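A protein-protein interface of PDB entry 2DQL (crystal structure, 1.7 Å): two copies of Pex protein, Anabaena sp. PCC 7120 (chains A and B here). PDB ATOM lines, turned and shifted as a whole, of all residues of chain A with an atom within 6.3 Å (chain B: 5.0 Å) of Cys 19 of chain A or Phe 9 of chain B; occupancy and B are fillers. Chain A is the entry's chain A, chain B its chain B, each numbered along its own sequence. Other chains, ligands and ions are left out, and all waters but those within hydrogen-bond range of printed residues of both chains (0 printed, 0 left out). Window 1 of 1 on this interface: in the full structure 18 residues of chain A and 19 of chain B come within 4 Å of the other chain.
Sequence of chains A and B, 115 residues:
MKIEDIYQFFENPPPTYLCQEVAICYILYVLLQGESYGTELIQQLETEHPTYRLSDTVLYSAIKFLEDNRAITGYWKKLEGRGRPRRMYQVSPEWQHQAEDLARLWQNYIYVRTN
The side-chain carboxylate (OE1) of Glu 21 of chain A sits at hydrogen-bond distance from the side-chain sulfur (SG) of Cys 19 of chain A (3.5 Å).
No position is printed for both chains.
Of the 6 pairs that touch across the chains among the printed residues, none has its exchanged pair printed and touching as well.
Cys 19 of chain A touches just one residue of chain B: Phe 9 (3.4 Å).
Printed residues of chain B within 4 Å of Ile 24 of chain A: Ile 6 (3.9 Å).
Of the printed residues of chain A, Phe 10 of chain B touches Tyr 109 (3.6 Å).
The nearest printed residue of chain A that does not touch Ile 6 of chain B is Val 22 of chain A (5.8 Å).
Of the 11 printed residues of chain A, 5 touch a printed residue of chain B.
Of the 10 printed residues of chain B, 3 touch a printed residue of chain A.
Hydrophobic or aromatic side chains of chain B that line the printed part of chain A: Ile 6, Phe 9 and Phe 10.
Among the printed residues, 6 pairs touch across the chains.
Among the printed residues, no Asp or Glu carboxylate lies within 4 Å of a Lys or Arg side-chain nitrogen of the other chain.
Cys 19 of chain A touches Phe 9 of chain B.
Glu 21 of chain A touches Ile 6 of chain B.
Glu 21 of chain A touches Phe 9 of chain B.
Phe 9 of chain B touches Val 22 of chain A.
Ile 6 of chain B touches Ile 24 of chain A.
Tyr 109 of chain A touches Phe 10 of chain B.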
ATOM      1  N   TYR A  17     -16.907 -21.320  -7.875  1.00  0.00           N
ATOM      2  CA  TYR A  17     -16.317 -20.210  -7.131  1.00  0.00           C
ATOM      3  C   TYR A  17     -14.821 -20.463  -7.059  1.00  0.00           C
ATOM      4  O   TYR A  17     -14.386 -21.533  -6.642  1.00  0.00           O
ATOM      5  CB  TYR A  17     -16.892 -20.115  -5.715  1.00  0.00           C
ATOM      6  CG  TYR A  17     -18.161 -19.309  -5.636  1.00  0.00           C
ATOM      7  CD1 TYR A  17     -19.364 -19.810  -6.136  1.00  0.00           C
ATOM      8  CD2 TYR A  17     -18.153 -18.018  -5.107  1.00  0.00           C
ATOM      9  CE1 TYR A  17     -20.527 -19.044  -6.110  1.00  0.00           C
ATOM     10  CE2 TYR A  17     -19.308 -17.246  -5.079  1.00  0.00           C
ATOM     11  CZ  TYR A  17     -20.490 -17.763  -5.583  1.00  0.00           C
ATOM     12  OH  TYR A  17     -21.627 -16.989  -5.576  1.00  0.00           O
ATOM     13  N   LEU A  18     -14.030 -19.479  -7.472  1.00  0.00           N
ATOM     14  CA  LEU A  18     -12.584 -19.632  -7.463  1.00  0.00           C
ATOM     15  C   LEU A  18     -12.020 -19.813  -6.061  1.00  0.00           C
ATOM     16  O   LEU A  18     -12.521 -19.227  -5.100  1.00  0.00           O
ATOM     17  CB  LEU A  18     -11.916 -18.404  -8.100  1.00  0.00           C
ATOM     18  CG  LEU A  18     -12.365 -17.966  -9.497  1.00  0.00           C
ATOM     19  CD1 LEU A  18     -11.470 -16.821  -9.967  1.00  0.00           C
ATOM     20  CD2 LEU A  18     -12.281 -19.138 -10.474  1.00  0.00           C
ATOM     21  N   CYS A  19     -10.980 -20.631  -5.944  1.00  0.00           N
ATOM     22  CA  CYS A  19     -10.318 -20.817  -4.662  1.00  0.00           C
ATOM     23  C   CYS A  19      -9.216 -19.763  -4.690  1.00  0.00           C
ATOM     24  O   CYS A  19      -8.978 -19.151  -5.735  1.00  0.00           O
ATOM     25  CB  CYS A  19      -9.721 -22.220  -4.535  1.00  0.00           C
ATOM     26  SG  CYS A  19      -8.482 -22.646  -5.773  1.00  0.00           S
ATOM     27  N   GLN A  20      -8.545 -19.558  -3.564  1.00  0.00           N
ATOM     28  CA  GLN A  20      -7.501 -18.540  -3.470  1.00  0.00           C
ATOM     29  C   GLN A  20      -6.394 -18.628  -4.516  1.00  0.00           C
ATOM     30  O   GLN A  20      -6.046 -17.623  -5.143  1.00  0.00           O
ATOM     31  CB  GLN A  20      -6.873 -18.556  -2.072  1.00  0.00           C
ATOM     32  CG  GLN A  20      -5.999 -17.341  -1.783  1.00  0.00           C
ATOM     33  CD  GLN A  20      -5.404 -17.371  -0.388  1.00  0.00           C
ATOM     34  OE1 GLN A  20      -6.102 -17.646   0.588  1.00  0.00           O
ATOM     35  NE2 GLN A  20      -4.109 -17.085  -0.287  1.00  0.00           N
ATOM     36  N   GLU A  21      -5.839 -19.819  -4.712  1.00  0.00           N
ATOM     37  CA  GLU A  21      -4.762 -19.994  -5.673  1.00  0.00           C
ATOM     38  C   GLU A  21      -5.143 -19.536  -7.075  1.00  0.00           C
ATOM     39  O   GLU A  21      -4.359 -18.866  -7.750  1.00  0.00           O
ATOM     40  CB  GLU A  21      -4.310 -21.459  -5.702  1.00  0.00           C
ATOM     41  CG  GLU A  21      -3.724 -21.948  -4.382  1.00  0.00           C
ATOM     42  CD  GLU A  21      -4.756 -22.558  -3.440  1.00  0.00           C
ATOM     43  OE1 GLU A  21      -5.930 -22.129  -3.443  1.00  0.00           O
ATOM     44  OE2 GLU A  21      -4.377 -23.469  -2.675  1.00  0.00           O
ATOM     45  N   VAL A  22      -6.346 -19.892  -7.510  1.00  0.00           N
ATOM     46  CA  VAL A  22      -6.816 -19.515  -8.835  1.00  0.00           C
ATOM     47  C   VAL A  22      -7.160 -18.024  -8.887  1.00  0.00           C
ATOM     48  O   VAL A  22      -6.833 -17.340  -9.851  1.00  0.00           O
ATOM     49  CB  VAL A  22      -8.056 -20.341  -9.243  1.00  0.00           C
ATOM     50  CG1 VAL A  22      -8.557 -19.890 -10.613  1.00  0.00           C
ATOM     51  CG2 VAL A  22      -7.696 -21.830  -9.272  1.00  0.00           C
ATOM     52  N   ALA A  23      -7.807 -17.519  -7.842  1.00  0.00           N
ATOM     53  CA  ALA A  23      -8.179 -16.103  -7.797  1.00  0.00           C
ATOM     54  C   ALA A  23      -6.950 -15.198  -7.885  1.00  0.00           C
ATOM     55  O   ALA A  23      -6.998 -14.140  -8.513  1.00  0.00           O
ATOM     56  CB  ALA A  23      -8.952 -15.809  -6.521  1.00  0.00           C
ATOM     57  N   ILE A  24      -5.857 -15.611  -7.251  1.00  0.00           N
ATOM     58  CA  ILE A  24      -4.630 -14.822  -7.282  1.00  0.00           C
ATOM     59  C   ILE A  24      -4.153 -14.663  -8.727  1.00  0.00           C
ATOM     60  O   ILE A  24      -3.787 -13.566  -9.151  1.00  0.00           O
ATOM     61  CB  ILE A  24      -3.522 -15.496  -6.445  1.00  0.00           C
ATOM     62  CG1 ILE A  24      -3.853 -15.381  -4.952  1.00  0.00           C
ATOM     63  CG2 ILE A  24      -2.164 -14.876  -6.761  1.00  0.00           C
ATOM     64  CD1 ILE A  24      -2.935 -16.222  -4.058  1.00  0.00           C
ATOM     65  N   LEU A  54     -16.443 -15.112  -8.025  1.00  0.00           N
ATOM     66  CA  LEU A  54     -15.384 -14.793  -7.080  1.00  0.00           C
ATOM     67  C   LEU A  54     -16.061 -14.190  -5.862  1.00  0.00           C
ATOM     68  O   LEU A  54     -16.723 -13.156  -5.966  1.00  0.00           O
ATOM     69  CB  LEU A  54     -14.392 -13.787  -7.676  1.00  0.00           C
ATOM     70  CG  LEU A  54     -13.302 -13.300  -6.709  1.00  0.00           C
ATOM     71  CD1 LEU A  54     -12.504 -14.473  -6.154  1.00  0.00           C
ATOM     72  CD2 LEU A  54     -12.382 -12.326  -7.441  1.00  0.00           C
ATOM     73  N   VAL A  58     -12.776 -14.689  -0.849  1.00  0.00           N
ATOM     74  CA  VAL A  58     -11.609 -15.156  -1.583  1.00  0.00           C
ATOM     75  C   VAL A  58     -10.892 -13.972  -2.235  1.00  0.00           C
ATOM     76  O   VAL A  58      -9.667 -13.949  -2.301  1.00  0.00           O
ATOM     77  CB  VAL A  58     -11.994 -16.199  -2.653  1.00  0.00           C
ATOM     78  CG1 VAL A  58     -10.766 -16.578  -3.484  1.00  0.00           C
ATOM     79  CG2 VAL A  58     -12.565 -17.442  -1.963  1.00  0.00           C
ATOM     80  N   TYR A 109      -5.945 -22.564 -17.191  1.00  0.00           N
ATOM     81  CA  TYR A 109      -6.946 -23.124 -16.291  1.00  0.00           C
ATOM     82  C   TYR A 109      -8.360 -22.912 -16.824  1.00  0.00           C
ATOM     83  O   TYR A 109      -9.183 -23.832 -16.829  1.00  0.00           O
ATOM     84  CB  TYR A 109      -6.822 -22.460 -14.919  1.00  0.00           C
ATOM     85  CG  TYR A 109      -7.888 -22.854 -13.923  1.00  0.00           C
ATOM     86  CD1 TYR A 109      -7.767 -24.016 -13.162  1.00  0.00           C
ATOM     87  CD2 TYR A 109      -9.009 -22.049 -13.725  1.00  0.00           C
ATOM     88  CE1 TYR A 109      -8.735 -24.363 -12.219  1.00  0.00           C
ATOM     89  CE2 TYR A 109      -9.983 -22.388 -12.786  1.00  0.00           C
ATOM     90  CZ  TYR A 109      -9.836 -23.542 -12.037  1.00  0.00           C
ATOM     91  OH  TYR A 109     -10.777 -23.855 -11.083  1.00  0.00           O
ATOM     92  N   ASP B   5       3.007 -22.617  -3.636  1.00  0.00           N
ATOM     93  CA  ASP B   5       1.750 -23.325  -3.429  1.00  0.00           C
ATOM     94  C   ASP B   5       0.815 -23.075  -4.600  1.00  0.00           C
ATOM     95  O   ASP B   5      -0.028 -23.908  -4.919  1.00  0.00           O
ATOM     96  CB  ASP B   5       1.070 -22.874  -2.134  1.00  0.00           C
ATOM     97  CG  ASP B   5       1.879 -23.216  -0.903  1.00  0.00           C
ATOM     98  OD1 ASP B   5       2.345 -24.373  -0.803  1.00  0.00           O
ATOM     99  OD2 ASP B   5       2.043 -22.335  -0.034  1.00  0.00           O
ATOM    100  N   ILE B   6       0.961 -21.919  -5.238  1.00  0.00           N
ATOM    101  CA  ILE B   6       0.117 -21.600  -6.378  1.00  0.00           C
ATOM    102  C   ILE B   6       0.470 -22.537  -7.523  1.00  0.00           C
ATOM    103  O   ILE B   6      -0.408 -23.133  -8.142  1.00  0.00           O
ATOM    104  CB  ILE B   6       0.311 -20.140  -6.827  1.00  0.00           C
ATOM    105  CG1 ILE B   6      -0.012 -19.201  -5.664  1.00  0.00           C
ATOM    106  CG2 ILE B   6      -0.591 -19.838  -8.012  1.00  0.00           C
ATOM    107  CD1 ILE B   6       0.320 -17.741  -5.938  1.00  0.00           C
ATOM    108  N   TYR B   7       1.761 -22.669  -7.801  1.00  0.00           N
ATOM    109  CA  TYR B   7       2.213 -23.550  -8.868  1.00  0.00           C
ATOM    110  C   TYR B   7       1.811 -24.993  -8.583  1.00  0.00           C
ATOM    111  O   TYR B   7       1.364 -25.710  -9.480  1.00  0.00           O
ATOM    112  CB  TYR B   7       3.729 -23.451  -9.023  1.00  0.00           C
ATOM    113  CG  TYR B   7       4.161 -22.218  -9.775  1.00  0.00           C
ATOM    114  CD1 TYR B   7       3.939 -22.109 -11.148  1.00  0.00           C
ATOM    115  CD2 TYR B   7       4.767 -21.151  -9.115  1.00  0.00           C
ATOM    116  CE1 TYR B   7       4.311 -20.965 -11.849  1.00  0.00           C
ATOM    117  CE2 TYR B   7       5.142 -19.999  -9.807  1.00  0.00           C
ATOM    118  CZ  TYR B   7       4.911 -19.916 -11.173  1.00  0.00           C
ATOM    119  OH  TYR B   7       5.282 -18.790 -11.867  1.00  0.00           O
ATOM    120  N   GLN B   8       1.968 -25.407  -7.331  1.00  0.00           N
ATOM    121  CA  GLN B   8       1.615 -26.764  -6.924  1.00  0.00           C
ATOM    122  C   GLN B   8       0.141 -27.051  -7.173  1.00  0.00           C
ATOM    123  O   GLN B   8      -0.221 -28.150  -7.591  1.00  0.00           O
ATOM    124  CB  GLN B   8       1.933 -26.976  -5.442  1.00  0.00           C
ATOM    125  CG  GLN B   8       3.410 -27.156  -5.130  1.00  0.00           C
ATOM    126  CD  GLN B   8       4.016 -28.339  -5.861  1.00  0.00           C
ATOM    127  OE1 GLN B   8       3.424 -29.418  -5.916  1.00  0.00           O
ATOM    128  NE2 GLN B   8       5.206 -28.146  -6.419  1.00  0.00           N
ATOM    129  N   PHE B   9      -0.706 -26.060  -6.914  1.00  0.00           N
ATOM    130  CA  PHE B   9      -2.142 -26.217  -7.110  1.00  0.00           C
ATOM    131  C   PHE B   9      -2.468 -26.653  -8.533  1.00  0.00           C
ATOM    132  O   PHE B   9      -3.336 -27.501  -8.752  1.00  0.00           O
ATOM    133  CB  PHE B   9      -2.874 -24.905  -6.820  1.00  0.00           C
ATOM    134  CG  PHE B   9      -4.352 -24.986  -7.050  1.00  0.00           C
ATOM    135  CD1 PHE B   9      -5.209 -25.390  -6.030  1.00  0.00           C
ATOM    136  CD2 PHE B   9      -4.885 -24.716  -8.306  1.00  0.00           C
ATOM    137  CE1 PHE B   9      -6.576 -25.526  -6.265  1.00  0.00           C
ATOM    138  CE2 PHE B   9      -6.248 -24.851  -8.549  1.00  0.00           C
ATOM    139  CZ  PHE B   9      -7.095 -25.258  -7.525  1.00  0.00           C
ATOM    140  N   PHE B  10      -1.775 -26.060  -9.498  1.00  0.00           N
ATOM    141  CA  PHE B  10      -1.992 -26.375 -10.902  1.00  0.00           C
ATOM    142  C   PHE B  10      -1.224 -27.618 -11.330  1.00  0.00           C
ATOM    143  O   PHE B  10      -1.691 -28.376 -12.177  1.00  0.00           O
ATOM    144  CB  PHE B  10      -1.586 -25.180 -11.764  1.00  0.00           C
ATOM    145  CG  PHE B  10      -2.472 -23.981 -11.581  1.00  0.00           C
ATOM    146  CD1 PHE B  10      -3.719 -23.926 -12.193  1.00  0.00           C
ATOM    147  CD2 PHE B  10      -2.078 -22.925 -10.769  1.00  0.00           C
ATOM    148  CE1 PHE B  10      -4.563 -22.836 -11.999  1.00  0.00           C
ATOM    149  CE2 PHE B  10      -2.914 -21.831 -10.569  1.00  0.00           C
ATOM    150  CZ  PHE B  10      -4.159 -21.787 -11.185  1.00  0.00           C
ATOM    151  N   GLU B  11      -0.051 -27.822 -10.735  1.00  0.00           N
ATOM    152  CA  GLU B  11       0.789 -28.977 -11.045  1.00  0.00           C
ATOM    153  C   GLU B  11       0.134 -30.258 -10.539  1.00  0.00           C
ATOM    154  O   GLU B  11      -0.038 -31.218 -11.292  1.00  0.00           O
ATOM    155  CB  GLU B  11       2.167 -28.830 -10.388  1.00  0.00           C
ATOM    156  CG  GLU B  11       2.992 -27.653 -10.888  1.00  0.00           C
ATOM    157  CD  GLU B  11       4.386 -27.619 -10.278  1.00  0.00           C
ATOM    158  OE1 GLU B  11       4.500 -27.508  -9.036  1.00  0.00           O
ATOM    159  OE2 GLU B  11       5.370 -27.704 -11.041  1.00  0.00           O
ATOM    160  N   ASN B  12      -0.222 -30.256  -9.258  1.00  0.00           N
ATOM    161  CA  ASN B  12      -0.858 -31.404  -8.619  1.00  0.00           C
ATOM    162  C   ASN B  12      -2.183 -30.947  -8.015  1.00  0.00           C
ATOM    163  O   ASN B  12      -2.258 -30.624  -6.829  1.00  0.00           O
ATOM    164  CB  ASN B  12       0.057 -31.962  -7.526  1.00  0.00           C
ATOM    165  CG  ASN B  12       1.422 -32.361  -8.062  1.00  0.00           C
ATOM    166  OD1 ASN B  12       1.528 -33.208  -8.950  1.00  0.00           O
ATOM    167  ND2 ASN B  12       2.473 -31.751  -7.524  1.00  0.00           N
ATOM    168  N   PRO B  13      -3.247 -30.916  -8.835  1.00  0.00           N
ATOM    169  CA  PRO B  13      -4.590 -30.497  -8.421  1.00  0.00           C
ATOM    170  C   PRO B  13      -5.072 -31.206  -7.167  1.00  0.00           C
ATOM    171  O   PRO B  13      -4.999 -32.432  -7.071  1.00  0.00           O
ATOM    172  CB  PRO B  13      -5.452 -30.852  -9.629  1.00  0.00           C
ATOM    173  CG  PRO B  13      -4.497 -30.761 -10.778  1.00  0.00           C
ATOM    174  CD  PRO B  13      -3.267 -31.423 -10.217  1.00  0.00           C
ATOM    175  N   PRO B  14      -5.561 -30.446  -6.178  1.00  0.00           N
ATOM    176  CA  PRO B  14      -6.042 -31.094  -4.960  1.00  0.00           C
ATOM    177  C   PRO B  14      -7.331 -31.855  -5.266  1.00  0.00           C
ATOM    178  O   PRO B  14      -7.967 -31.628  -6.293  1.00  0.00           O
ATOM    179  CB  PRO B  14      -6.263 -29.921  -4.012  1.00  0.00           C
ATOM    180  CG  PRO B  14      -6.658 -28.818  -4.937  1.00  0.00           C
ATOM    181  CD  PRO B  14      -5.682 -28.978  -6.080  1.00  0.00           C
